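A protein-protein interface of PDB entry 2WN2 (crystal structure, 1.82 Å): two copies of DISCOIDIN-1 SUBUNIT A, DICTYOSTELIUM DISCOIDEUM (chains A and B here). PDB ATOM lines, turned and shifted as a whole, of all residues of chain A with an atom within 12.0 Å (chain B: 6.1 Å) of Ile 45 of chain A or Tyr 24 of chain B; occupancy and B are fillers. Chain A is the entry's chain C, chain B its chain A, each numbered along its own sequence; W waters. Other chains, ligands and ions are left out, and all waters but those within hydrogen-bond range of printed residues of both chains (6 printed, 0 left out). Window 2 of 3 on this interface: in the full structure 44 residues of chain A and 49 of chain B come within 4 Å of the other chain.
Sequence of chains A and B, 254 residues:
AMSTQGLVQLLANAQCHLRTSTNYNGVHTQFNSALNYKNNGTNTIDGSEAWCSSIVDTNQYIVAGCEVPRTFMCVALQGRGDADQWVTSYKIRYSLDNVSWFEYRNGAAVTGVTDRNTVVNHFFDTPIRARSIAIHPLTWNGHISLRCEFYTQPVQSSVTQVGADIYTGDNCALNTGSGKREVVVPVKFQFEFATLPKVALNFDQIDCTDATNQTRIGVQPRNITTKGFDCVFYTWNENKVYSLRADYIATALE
O of Ser 54 of chain B is in hydrogen-bond range of ND2 of Asn 40 of chain A (3.4 Å).
OD2 of Asp 46 of chain A is in hydrogen-bond range of OG of Ser 54 of chain B.
The side-chain amide oxygen (OD1) of Asn 23 of chain B sits at hydrogen-bond distance from the indole nitrogen (NE1) of Trp 51 of chain B (2.9 Å).
The side-chain amide oxygen of Asn 25 of chain A lies within hydrogen-bond range of the backbone NH of Val 27 of chain A (2.5 Å).
The backbone NH (N) of Asn 40 of chain A sits at hydrogen-bond distance from the side-chain carboxylate (OD2) of Asp 46 of chain A.
The side-chain amide oxygen of Asn 43 of chain A sits close to the backbone NH of Ile 45 of chain A (3.3 Å).
Among the printed residues, merely in contact across the chains: Gly 26 of chain A with Gly 26 of chain B (3.5 Å), Val 27 of chain A with Asn 25 of chain B (3.7 Å), Val 27 of chain A with Gly 26 of chain B (3.2 Å), Phe 31 of chain A with Asn 23 of chain B (3.5 Å), Phe 31 of chain A with Thr 29 of chain B (3.5 Å), Lys 38 of chain A with Thr 22 of chain B (3.7 Å), Ile 45 of chain A with Tyr 24 of chain B (3.4 Å), Ile 45 of chain A with Asn 25 of chain B (3.6 Å), Asp 46 of chain A with Asn 23 of chain B (3.4 Å) and Asp 46 of chain A with Tyr 24 of chain B (3.6 Å).
Of the printed residues of chain B, Gly 26 of chain A touches Gly 26.
Printed residues of chain B within 4 Å of Ile 45 of chain A: Tyr 24 and Asn 25.
Ser 48 of chain A touches none of the printed residues of chain B.
Asn 23 of chain B touches two residues of chain A.
Of chain A, only Ile 45 and Asp 46 come within 4 Å of Tyr 24 of chain B.
Asn 25 of chain B touches just these residues of chain A: Val 27 (3.7 Å) and Ile 45 (3.6 Å).
Gly 26 of chain B touches two residues of chain A.
Of the printed residues of chain A, Thr 29 of chain B touches Phe 31.
No residue of chain A comes within 4 Å of Cys 52 of chain B.
The nearest residue of chain B that does not touch Ile 45 of chain A is Gly 26 of chain B (5.1 Å).
The nearest printed residue of chain B that does not touch Lys 38 of chain A is Ser 54 of chain B (7.4 Å).
Hydrophobic or aromatic side chains of chain A that line the printed part of chain B: Val 27, Phe 31 and Ile 45.
Of the 12 printed residues of chain B, 7 touch a printed residue of chain A.
Printed residues of chain B that touch a printed residue of chain A: Thr 22, Asn 23, Tyr 24, Asn 25, Gly 26, Thr 29 and Ser 54.
Hydrophobic or aromatic side chains of chain B within 4 Å of the printed part of chain A: Tyr 24.
Along chain B the printed residues that touch a printed residue of chain A span positions 22 to 54.
Among the printed residues, no Asp or Glu carboxylate lies within 4 Å of a Lys or Arg side-chain nitrogen of the other chain.
Gly 26 of chain B touches its own counterpart, Gly 26 of chain A.
Positions printed for both chains: 24, 25, 26, 28 and 29.
Of the 12 pairs that touch across the chains among the printed residues, 1 has its exchanged pair printed and touching as well.
Water W3 lies within hydrogen-bond range of O of Ser 54 of chain B (2.6 Å), ND2 of Asn 43 of chain A (3.3 Å) and ND2 of Asn 40 of chain A (3.5 Å).
Water W4 lies within hydrogen-bond range of OH of Tyr 37 of chain A, OD1 of Asn 32 of chain A and N of Asn 23 of chain B.
Water W2 lies within hydrogen-bond range of OG of Ser 54 of chain B, O of Tyr 24 of chain B and ND2 of Asn 43 of chain A.
Water W1 lies within hydrogen-bond range of O of Asn 23 of chain B (2.9 Å) and O of Asp 46 of chain A (3.0 Å).
Water W5 lies within hydrogen-bond range of the backbone carbonyl oxygen of Gly 26 of chain B (3.3 Å) and the backbone carbonyl oxygen of Gly 26 of chain A (3.3 Å).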
ATOM      1  N   TYR A  24      -6.748 -33.541  10.681  1.00  0.00           N
ATOM      2  CA  TYR A  24      -6.988 -32.263   9.966  1.00  0.00           C
ATOM      3  C   TYR A  24      -5.784 -31.856   9.075  1.00  0.00           C
ATOM      4  O   TYR A  24      -5.935 -31.506   7.914  1.00  0.00           O
ATOM      5  CB  TYR A  24      -7.291 -31.214  10.997  1.00  0.00           C
ATOM      6  CG  TYR A  24      -7.691 -29.874  10.417  1.00  0.00           C
ATOM      7  CD1 TYR A  24      -8.903 -29.710   9.770  1.00  0.00           C
ATOM      8  CD2 TYR A  24      -6.826 -28.784  10.492  1.00  0.00           C
ATOM      9  CE1 TYR A  24      -9.298 -28.454   9.242  1.00  0.00           C
ATOM     10  CE2 TYR A  24      -7.219 -27.521   9.980  1.00  0.00           C
ATOM     11  CZ  TYR A  24      -8.429 -27.381   9.349  1.00  0.00           C
ATOM     12  OH  TYR A  24      -8.788 -26.151   8.835  1.00  0.00           O
ATOM     13  N   ASN A  25      -4.591 -31.986   9.649  1.00  0.00           N
ATOM     14  CA  ASN A  25      -3.313 -31.868   8.955  1.00  0.00           C
ATOM     15  C   ASN A  25      -2.267 -32.553   9.826  1.00  0.00           C
ATOM     16  O   ASN A  25      -2.611 -33.323  10.747  1.00  0.00           O
ATOM     17  CB  ASN A  25      -2.895 -30.399   8.839  1.00  0.00           C
ATOM     18  CG  ASN A  25      -2.400 -29.835  10.182  1.00  0.00           C
ATOM     19  OD1 ASN A  25      -2.349 -30.451  11.170  1.00  0.00           O
ATOM     20  ND2 ASN A  25      -2.049 -28.617  10.120  1.00  0.00           N
ATOM     21  N   GLY A  26      -0.991 -32.352   9.509  1.00  0.00           N
ATOM     22  CA  GLY A  26       0.064 -33.078  10.190  1.00  0.00           C
ATOM     23  C   GLY A  26       0.454 -32.511  11.542  1.00  0.00           C
ATOM     24  O   GLY A  26       1.316 -33.059  12.219  1.00  0.00           O
ATOM     25  N   VAL A  27      -0.184 -31.422  11.956  1.00  0.00           N
ATOM     26  CA  VAL A  27       0.008 -30.853  13.301  1.00  0.00           C
ATOM     27  C   VAL A  27      -1.316 -30.871  14.089  1.00  0.00           C
ATOM     28  O   VAL A  27      -1.488 -30.164  15.074  1.00  0.00           O
ATOM     29  CB  VAL A  27       0.726 -29.458  13.298  1.00  0.00           C
ATOM     30  CG1 VAL A  27       2.205 -29.588  12.796  1.00  0.00           C
ATOM     31  CG2 VAL A  27      -0.037 -28.404  12.451  1.00  0.00           C
ATOM     32  N   HIS A  28      -2.254 -31.717  13.657  1.00  0.00           N
ATOM     33  CA  HIS A  28      -3.456 -31.952  14.432  1.00  0.00           C
ATOM     34  C   HIS A  28      -3.656 -33.445  14.656  1.00  0.00           C
ATOM     35  O   HIS A  28      -4.807 -33.907  14.747  1.00  0.00           O
ATOM     36  CB  HIS A  28      -4.685 -31.392  13.716  1.00  0.00           C
ATOM     37  CG  HIS A  28      -4.712 -29.900  13.583  1.00  0.00           C
ATOM     38  ND1 HIS A  28      -3.825 -29.196  12.791  1.00  0.00           N
ATOM     39  CD2 HIS A  28      -5.578 -28.984  14.087  1.00  0.00           C
ATOM     40  CE1 HIS A  28      -4.124 -27.901  12.855  1.00  0.00           C
ATOM     41  NE2 HIS A  28      -5.172 -27.748  13.648  1.00  0.00           N
ATOM     42  N   THR A  29      -2.551 -34.201  14.697  1.00  0.00           N
ATOM     43  CA  THR A  29      -2.653 -35.667  14.734  1.00  0.00           C
ATOM     44  C   THR A  29      -2.758 -36.186  16.161  1.00  0.00           C
ATOM     45  O   THR A  29      -2.640 -35.421  17.138  1.00  0.00           O
ATOM     46  CB  THR A  29      -1.422 -36.324  14.076  1.00  0.00           C
ATOM     47  OG1 THR A  29      -0.308 -36.215  14.979  1.00  0.00           O
ATOM     48  CG2 THR A  29      -1.076 -35.666  12.718  1.00  0.00           C
ATOM     49  N   PHE A  31      -0.431 -37.431  17.741  1.00  0.00           N
ATOM     50  CA  PHE A  31       0.715 -37.000  18.548  1.00  0.00           C
ATOM     51  C   PHE A  31       0.332 -35.986  19.597  1.00  0.00           C
ATOM     52  O   PHE A  31       1.082 -35.810  20.588  1.00  0.00           O
ATOM     53  CB  PHE A  31       1.805 -36.390  17.657  1.00  0.00           C
ATOM     54  CG  PHE A  31       2.552 -37.373  16.776  1.00  0.00           C
ATOM     55  CD1 PHE A  31       2.862 -38.666  17.200  1.00  0.00           C
ATOM     56  CD2 PHE A  31       3.032 -36.954  15.531  1.00  0.00           C
ATOM     57  CE1 PHE A  31       3.590 -39.523  16.362  1.00  0.00           C
ATOM     58  CE2 PHE A  31       3.746 -37.814  14.704  1.00  0.00           C
ATOM     59  CZ  PHE A  31       4.043 -39.086  15.124  1.00  0.00           C
ATOM     60  N   ASN A  32      -0.806 -35.299  19.388  1.00  0.00           N
ATOM     61  CA  ASN A  32      -1.257 -34.187  20.240  1.00  0.00           C
ATOM     62  C   ASN A  32      -2.463 -34.579  21.105  1.00  0.00           C
ATOM     63  O   ASN A  32      -3.190 -33.709  21.568  1.00  0.00           O
ATOM     64  CB  ASN A  32      -1.618 -32.979  19.367  1.00  0.00           C
ATOM     65  CG  ASN A  32      -0.450 -32.485  18.521  1.00  0.00           C
ATOM     66  OD1 ASN A  32       0.615 -33.058  18.529  1.00  0.00           O
ATOM     67  ND2 ASN A  32      -0.646 -31.355  17.845  1.00  0.00           N
ATOM     68  N   TYR A  37      -2.246 -32.329  27.100  1.00  0.00           N
ATOM     69  CA  TYR A  37      -1.217 -31.963  26.125  1.00  0.00           C
ATOM     70  C   TYR A  37      -1.319 -30.458  25.926  1.00  0.00           C
ATOM     71  O   TYR A  37      -2.406 -29.943  25.693  1.00  0.00           O
ATOM     72  CB  TYR A  37      -1.455 -32.686  24.789  1.00  0.00           C
ATOM     73  CG  TYR A  37      -0.596 -32.154  23.657  1.00  0.00           C
ATOM     74  CD1 TYR A  37      -1.067 -31.138  22.853  1.00  0.00           C
ATOM     75  CD2 TYR A  37       0.659 -32.655  23.394  1.00  0.00           C
ATOM     76  CE1 TYR A  37      -0.326 -30.614  21.809  1.00  0.00           C
ATOM     77  CE2 TYR A  37       1.454 -32.121  22.320  1.00  0.00           C
ATOM     78  CZ  TYR A  37       0.945 -31.094  21.560  1.00  0.00           C
ATOM     79  OH  TYR A  37       1.628 -30.519  20.509  1.00  0.00           O
ATOM     80  N   LYS A  38      -0.195 -29.790  26.019  1.00  0.00           N
ATOM     81  CA  LYS A  38      -0.091 -28.349  25.719  1.00  0.00           C
ATOM     82  C   LYS A  38       1.137 -28.132  24.861  1.00  0.00           C
ATOM     83  O   LYS A  38       2.143 -28.833  25.013  1.00  0.00           O
ATOM     84  CB  LYS A  38       0.045 -27.565  27.039  1.00  0.00           C
ATOM     85  CG  LYS A  38      -1.290 -27.547  27.846  1.00  0.00           C
ATOM     86  CD  LYS A  38      -1.145 -26.688  29.095  1.00  0.00           C
ATOM     87  CE  LYS A  38      -0.805 -27.493  30.365  1.00  0.00           C
ATOM     88  NZ  LYS A  38       0.663 -27.474  30.707  1.00  0.00           N
ATOM     89  N   ASN A  39       1.065 -27.153  23.965  1.00  0.00           N
ATOM     90  CA  ASN A  39       2.178 -26.899  23.088  1.00  0.00           C
ATOM     91  C   ASN A  39       2.592 -25.431  23.133  1.00  0.00           C
ATOM     92  O   ASN A  39       2.268 -24.709  24.100  1.00  0.00           O
ATOM     93  CB  ASN A  39       1.845 -27.431  21.680  1.00  0.00           C
ATOM     94  CG  ASN A  39       0.725 -26.715  21.014  1.00  0.00           C
ATOM     95  OD1 ASN A  39       0.210 -25.707  21.495  1.00  0.00           O
ATOM     96  ND2 ASN A  39       0.313 -27.258  19.855  1.00  0.00           N
ATOM     97  N   ASN A  40       3.319 -24.988  22.112  1.00  0.00           N
ATOM     98  CA  ASN A  40       3.805 -23.616  22.048  1.00  0.00           C
ATOM     99  C   ASN A  40       2.677 -22.681  21.613  1.00  0.00           C
ATOM    100  O   ASN A  40       2.265 -22.666  20.449  1.00  0.00           O
ATOM    101  CB  ASN A  40       4.999 -23.529  21.106  1.00  0.00           C
ATOM    102  CG  ASN A  40       5.746 -22.222  21.240  1.00  0.00           C
ATOM    103  OD1 ASN A  40       5.141 -21.187  21.508  1.00  0.00           O
ATOM    104  ND2 ASN A  40       7.061 -22.251  21.008  1.00  0.00           N
ATOM    105  N   GLY A  41       2.178 -21.927  22.581  1.00  0.00           N
ATOM    106  CA  GLY A  41       1.102 -20.971  22.369  1.00  0.00           C
ATOM    107  C   GLY A  41       1.571 -19.700  21.668  1.00  0.00           C
ATOM    108  O   GLY A  41       0.739 -18.887  21.283  1.00  0.00           O
ATOM    109  N   THR A  42       2.873 -19.511  21.507  1.00  0.00           N
ATOM    110  CA  THR A  42       3.390 -18.324  20.794  1.00  0.00           C
ATOM    111  C   THR A  42       3.734 -18.634  19.308  1.00  0.00           C
ATOM    112  O   THR A  42       4.000 -17.720  18.518  1.00  0.00           O
ATOM    113  CB  THR A  42       4.589 -17.676  21.514  1.00  0.00           C
ATOM    114  OG1 THR A  42       5.777 -18.426  21.274  1.00  0.00           O
ATOM    115  CG2 THR A  42       4.361 -17.605  22.996  1.00  0.00           C
ATOM    116  N   ASN A  43       3.658 -19.903  18.909  1.00  0.00           N
ATOM    117  CA  ASN A  43       4.009 -20.296  17.567  1.00  0.00           C
ATOM    118  C   ASN A  43       2.863 -21.119  16.985  1.00  0.00           C
ATOM    119  O   ASN A  43       2.414 -22.086  17.579  1.00  0.00           O
ATOM    120  CB  ASN A  43       5.319 -21.077  17.591  1.00  0.00           C
ATOM    121  CG  ASN A  43       5.966 -21.139  16.235  1.00  0.00           C
ATOM    122  OD1 ASN A  43       5.293 -20.897  15.240  1.00  0.00           O
ATOM    123  ND2 ASN A  43       7.235 -21.562  16.171  1.00  0.00           N
ATOM    124  N   THR A  44       2.322 -20.706  15.861  1.00  0.00           N
ATOM    125  CA  THR A  44       1.173 -21.434  15.282  1.00  0.00           C
ATOM    126  C   THR A  44       1.554 -22.767  14.648  1.00  0.00           C
ATOM    127  O   THR A  44       0.682 -23.604  14.398  1.00  0.00           O
ATOM    128  CB  THR A  44       0.462 -20.554  14.227  1.00  0.00           C
ATOM    129  OG1 THR A  44       1.392 -20.248  13.183  1.00  0.00           O
ATOM    130  CG2 THR A  44      -0.034 -19.245  14.847  1.00  0.00           C
ATOM    131  N   ILE A  45       2.840 -22.958  14.325  1.00  0.00           N
ATOM    132  CA  ILE A  45       3.210 -24.007  13.405  1.00  0.00           C
ATOM    133  C   ILE A  45       3.083 -25.412  13.997  1.00  0.00           C
ATOM    134  O   ILE A  45       3.018 -26.397  13.227  1.00  0.00           O
ATOM    135  CB  ILE A  45       4.616 -23.810  12.782  1.00  0.00           C
ATOM    136  CG1 ILE A  45       5.750 -24.061  13.790  1.00  0.00           C
ATOM    137  CG2 ILE A  45       4.669 -22.384  12.144  1.00  0.00           C
ATOM    138  CD1 ILE A  45       7.160 -24.118  13.152  1.00  0.00           C
ATOM    139  N   ASP A  46       3.107 -25.498  15.327  1.00  0.00           N
ATOM    140  CA  ASP A  46       2.963 -26.796  16.019  1.00  0.00           C
ATOM    141  C   ASP A  46       1.541 -27.265  16.219  1.00  0.00           C
ATOM    142  O   ASP A  46       1.358 -28.346  16.767  1.00  0.00           O
ATOM    143  CB  ASP A  46       3.757 -26.842  17.324  1.00  0.00           C
ATOM    144  CG  ASP A  46       3.257 -25.883  18.379  1.00  0.00           C
ATOM    145  OD1 ASP A  46       2.454 -24.958  18.106  1.00  0.00           O
ATOM    146  OD2 ASP A  46       3.718 -26.079  19.525  1.00  0.00           O
ATOM    147  N   GLY A  47       0.545 -26.497  15.757  1.00  0.00           N
ATOM    148  CA  GLY A  47      -0.826 -26.991  15.632  1.00  0.00           C
ATOM    149  C   GLY A  47      -1.666 -26.943  16.908  1.00  0.00           C
ATOM    150  O   GLY A  47      -1.471 -26.098  17.805  1.00  0.00           O
ATOM    151  N   SER A  48      -2.579 -27.903  16.996  1.00  0.00           N
ATOM    152  CA  SER A  48      -3.641 -27.931  17.972  1.00  0.00           C
ATOM    153  C   SER A  48      -3.276 -28.665  19.248  1.00  0.00           C
ATOM    154  O   SER A  48      -2.530 -29.629  19.218  1.00  0.00           O
ATOM    155  CB  SER A  48      -4.831 -28.631  17.369  1.00  0.00           C
ATOM    156  OG  SER A  48      -4.525 -29.936  16.894  1.00  0.00           O
ATOM    157  N   GLU A  49      -3.833 -28.211  20.373  1.00  0.00           N
ATOM    158  CA  GLU A  49      -3.720 -28.932  21.627  1.00  0.00           C
ATOM    159  C   GLU A  49      -4.856 -29.944  21.678  1.00  0.00           C
ATOM    160  O   GLU A  49      -5.784 -29.865  22.519  1.00  0.00           O
ATOM    161  CB  GLU A  49      -3.717 -27.978  22.823  1.00  0.00           C
ATOM    162  CG  GLU A  49      -2.489 -27.065  22.830  1.00  0.00           C
ATOM    163  CD  GLU A  49      -2.492 -26.033  23.973  1.00  0.00           C
ATOM    164  OE1 GLU A  49      -3.604 -25.561  24.383  1.00  0.00           O
ATOM    165  OE2 GLU A  49      -1.375 -25.693  24.408  1.00  0.00           O
ATOM    166  N   ALA A  50      -4.783 -30.875  20.732  1.00  0.00           N
ATOM    167  CA  ALA A  50      -5.779 -31.902  20.474  1.00  0.00           C
ATOM    168  C   ALA A  50      -5.466 -32.688  19.199  1.00  0.00           C
ATOM    169  O   ALA A  50      -4.760 -32.213  18.320  1.00  0.00           O
ATOM    170  CB  ALA A  50      -7.224 -31.286  20.331  1.00  0.00           C
ATOM    171  N   ARG A  80     -10.232 -29.325  23.256  1.00  0.00           N
ATOM    172  CA  ARG A  80      -9.036 -28.740  22.643  1.00  0.00           C
ATOM    173  C   ARG A  80      -8.561 -27.576  23.466  1.00  0.00           C
ATOM    174  O   ARG A  80      -9.349 -26.685  23.815  1.00  0.00           O
ATOM    175  CB  ARG A  80      -9.356 -28.272  21.224  1.00  0.00           C
ATOM    176  CG  ARG A  80      -8.158 -27.606  20.515  1.00  0.00           C
ATOM    177  CD  ARG A  80      -8.455 -27.396  19.021  1.00  0.00           C
ATOM    178  NE  ARG A  80      -7.409 -26.547  18.474  1.00  0.00           N
ATOM    179  CZ  ARG A  80      -7.299 -26.129  17.221  1.00  0.00           C
ATOM    180  NH1 ARG A  80      -8.193 -26.447  16.329  1.00  0.00           N
ATOM    181  NH2 ARG A  80      -6.238 -25.369  16.893  1.00  0.00           N
ATOM    182  N   ASP A  82      -6.569 -24.963  22.854  1.00  0.00           N
ATOM    183  CA  ASP A  82      -6.194 -23.665  22.266  1.00  0.00           C
ATOM    184  C   ASP A  82      -7.298 -23.095  21.416  1.00  0.00           C
ATOM    185  O   ASP A  82      -7.112 -22.014  20.856  1.00  0.00           O
ATOM    186  CB  ASP A  82      -4.886 -23.748  21.448  1.00  0.00           C
ATOM    187  CG  ASP A  82      -5.017 -24.657  20.214  1.00  0.00           C
ATOM    188  OD1 ASP A  82      -5.378 -25.851  20.363  1.00  0.00           O
ATOM    189  OD2 ASP A  82      -4.785 -24.189  19.070  1.00  0.00           O
ATOM    190  N   THR B  22       6.338 -32.248  22.751  1.00  0.00           N
ATOM    191  CA  THR B  22       5.932 -31.336  21.675  1.00  0.00           C
ATOM    192  C   THR B  22       6.794 -31.660  20.466  1.00  0.00           C
ATOM    193  O   THR B  22       7.898 -32.208  20.590  1.00  0.00           O
ATOM    194  CB  THR B  22       6.108 -29.813  22.013  1.00  0.00           C
ATOM    195  OG1 THR B  22       7.476 -29.516  22.244  1.00  0.00           O
ATOM    196  CG2 THR B  22       5.306 -29.413  23.186  1.00  0.00           C
ATOM    197  N   ASN B  23       6.276 -31.310  19.279  1.00  0.00           N
ATOM    198  CA  ASN B  23       6.956 -31.486  18.028  1.00  0.00           C
ATOM    199  C   ASN B  23       6.990 -30.110  17.304  1.00  0.00           C
ATOM    200  O   ASN B  23       5.948 -29.466  17.153  1.00  0.00           O
ATOM    201  CB  ASN B  23       6.141 -32.461  17.137  1.00  0.00           C
ATOM    202  CG  ASN B  23       6.132 -33.876  17.643  1.00  0.00           C
ATOM    203  OD1 ASN B  23       7.118 -34.319  18.239  1.00  0.00           O
ATOM    204  ND2 ASN B  23       5.054 -34.638  17.301  1.00  0.00           N
ATOM    205  N   TYR B  24       8.144 -29.730  16.800  1.00  0.00           N
ATOM    206  CA  TYR B  24       8.300 -28.415  16.171  1.00  0.00           C
ATOM    207  C   TYR B  24       7.225 -28.168  15.105  1.00  0.00           C
ATOM    208  O   TYR B  24       6.576 -27.100  15.035  1.00  0.00           O
ATOM    209  CB  TYR B  24       9.708 -28.298  15.584  1.00  0.00           C
ATOM    210  CG  TYR B  24      10.053 -26.926  15.036  1.00  0.00           C
ATOM    211  CD1 TYR B  24      10.232 -25.871  15.879  1.00  0.00           C
ATOM    212  CD2 TYR B  24      10.250 -26.732  13.658  1.00  0.00           C
ATOM    213  CE1 TYR B  24      10.536 -24.602  15.383  1.00  0.00           C
ATOM    214  CE2 TYR B  24      10.578 -25.520  13.158  1.00  0.00           C
ATOM    215  CZ  TYR B  24      10.714 -24.440  14.022  1.00  0.00           C
ATOM    216  OH  TYR B  24      11.067 -23.216  13.502  1.00  0.00           O
ATOM    217  N   ASN B  25       7.096 -29.122  14.205  1.00  0.00           N
ATOM    218  CA  ASN B  25       5.916 -29.240  13.356  1.00  0.00           C
ATOM    219  C   ASN B  25       5.793 -30.669  12.886  1.00  0.00           C
ATOM    220  O   ASN B  25       6.447 -31.580  13.410  1.00  0.00           O
ATOM    221  CB  ASN B  25       5.937 -28.200  12.188  1.00  0.00           C
ATOM    222  CG  ASN B  25       6.915 -28.542  11.076  1.00  0.00           C
ATOM    223  OD1 ASN B  25       7.530 -29.599  11.089  1.00  0.00           O
ATOM    224  ND2 ASN B  25       7.040 -27.626  10.056  1.00  0.00           N
ATOM    225  N   GLY B  26       5.000 -30.881  11.849  1.00  0.00           N
ATOM    226  CA  GLY B  26       4.653 -32.217  11.464  1.00  0.00           C
ATOM    227  C   GLY B  26       5.726 -32.978  10.713  1.00  0.00           C
ATOM    228  O   GLY B  26       5.508 -34.151  10.379  1.00  0.00           O
ATOM    229  N   HIS B  28       8.997 -32.689  11.965  1.00  0.00           N
ATOM    230  CA  HIS B  28      10.044 -32.743  12.979  1.00  0.00           C
ATOM    231  C   HIS B  28       9.649 -33.692  14.130  1.00  0.00           C
ATOM    232  O   HIS B  28      10.046 -33.477  15.289  1.00  0.00           O
ATOM    233  CB  HIS B  28      10.310 -31.342  13.564  1.00  0.00           C
ATOM    234  CG  HIS B  28      10.905 -30.370  12.589  1.00  0.00           C
ATOM    235  ND1 HIS B  28      10.206 -29.873  11.503  1.00  0.00           N
ATOM    236  CD2 HIS B  28      12.140 -29.809  12.534  1.00  0.00           C
ATOM    237  CE1 HIS B  28      10.998 -29.062  10.810  1.00  0.00           C
ATOM    238  NE2 HIS B  28      12.163 -28.983  11.428  1.00  0.00           N
ATOM    239  N   THR B  29       8.854 -34.721  13.815  1.00  0.00           N
ATOM    240  CA  THR B  29       8.181 -35.536  14.851  1.00  0.00           C
ATOM    241  C   THR B  29       9.031 -36.736  15.200  1.00  0.00           C
ATOM    242  O   THR B  29      10.116 -36.954  14.629  1.00  0.00           O
ATOM    243  CB  THR B  29       6.804 -36.068  14.375  1.00  0.00           C
ATOM    244  OG1 THR B  29       7.008 -37.119  13.419  1.00  0.00           O
ATOM    245  CG2 THR B  29       5.911 -34.962  13.765  1.00  0.00           C
ATOM    246  N   TRP B  51      13.887 -35.888  15.818  1.00  0.00           N
ATOM    247  CA  TRP B  51      12.761 -35.310  16.546  1.00  0.00           C
ATOM    248  C   TRP B  51      13.229 -33.966  17.110  1.00  0.00           C
ATOM    249  O   TRP B  51      14.293 -33.914  17.722  1.00  0.00           O
ATOM    250  CB  TRP B  51      12.247 -36.236  17.683  1.00  0.00           C
ATOM    251  CG  TRP B  51      11.381 -35.467  18.644  1.00  0.00           C
ATOM    252  CD1 TRP B  51      10.238 -34.813  18.356  1.00  0.00           C
ATOM    253  CD2 TRP B  51      11.695 -35.125  20.015  1.00  0.00           C
ATOM    254  NE1 TRP B  51       9.781 -34.171  19.459  1.00  0.00           N
ATOM    255  CE2 TRP B  51      10.654 -34.327  20.486  1.00  0.00           C
ATOM    256  CE3 TRP B  51      12.723 -35.472  20.887  1.00  0.00           C
ATOM    257  CZ2 TRP B  51      10.606 -33.822  21.813  1.00  0.00           C
ATOM    258  CZ3 TRP B  51      12.693 -34.957  22.203  1.00  0.00           C
ATOM    259  CH2 TRP B  51      11.626 -34.166  22.645  1.00  0.00           C
ATOM    260  N   CYS B  52      12.456 -32.887  16.879  1.00  0.00           N
ATOM    261  CA  CYS B  52      12.753 -31.552  17.443  1.00  0.00           C
ATOM    262  C   CYS B  52      11.521 -31.039  18.160  1.00  0.00           C
ATOM    263  O   CYS B  52      10.430 -31.135  17.640  1.00  0.00           O
ATOM    264  CB  CYS B  52      13.140 -30.581  16.314  1.00  0.00           C
ATOM    265  SG  CYS B  52      14.436 -31.193  15.212  1.00  0.00           S
ATOM    266  N   SER B  53      11.670 -30.526  19.371  1.00  0.00           N
ATOM    267  CA  SER B  53      10.562 -30.041  20.155  1.00  0.00           C
ATOM    268  C   SER B  53      10.035 -28.721  19.588  1.00  0.00           C
ATOM    269  O   SER B  53      10.715 -28.069  18.756  1.00  0.00           O
ATOM    270  CB  SER B  53      10.999 -29.813  21.625  1.00  0.00           C
ATOM    271  OG  SER B  53      11.918 -28.750  21.723  1.00  0.00           O
ATOM    272  N   SER B  54       8.843 -28.339  20.014  1.00  0.00           N
ATOM    273  CA  SER B  54       8.316 -27.022  19.703  1.00  0.00           C
ATOM    274  C   SER B  54       8.722 -26.011  20.767  1.00  0.00           C
ATOM    275  O   SER B  54       9.106 -24.887  20.455  1.00  0.00           O
ATOM    276  CB  SER B  54       6.814 -27.026  19.599  1.00  0.00           C
ATOM    277  OG  SER B  54       6.399 -25.756  19.162  1.00  0.00           O
ATOM    278  N   HIS B 143      19.071 -26.191  19.624  1.00  0.00           N
ATOM    279  CA  HIS B 143      17.669 -26.569  19.823  1.00  0.00           C
ATOM    280  C   HIS B 143      17.588 -27.983  20.423  1.00  0.00           C
ATOM    281  O   HIS B 143      18.552 -28.740  20.367  1.00  0.00           O
ATOM    282  CB  HIS B 143      16.974 -26.600  18.460  1.00  0.00           C
ATOM    283  CG  HIS B 143      15.486 -26.613  18.517  1.00  0.00           C
ATOM    284  ND1 HIS B 143      14.733 -25.467  18.615  1.00  0.00           N
ATOM    285  CD2 HIS B 143      14.604 -27.631  18.419  1.00  0.00           C
ATOM    286  CE1 HIS B 143      13.449 -25.786  18.610  1.00  0.00           C
ATOM    287  NE2 HIS B 143      13.348 -27.099  18.508  1.00  0.00           N
HETATM  288  O   HOH W   1       3.439 -30.351  16.083  1.00  0.00           O
HETATM  289  O   HOH W   2       7.017 -24.807  16.776  1.00  0.00           O
HETATM  290  O   HOH W   3       8.819 -23.455  18.289  1.00  0.00           O
HETATM  291  O   HOH W   4       3.225 -32.153  19.204  1.00  0.00           O
HETATM  292  O   HOH W   5       2.804 -35.778  11.171  1.00  0.00           O
HETATM  293  O   HOH W   6       3.001 -33.085  16.207  1.00  0.00           O
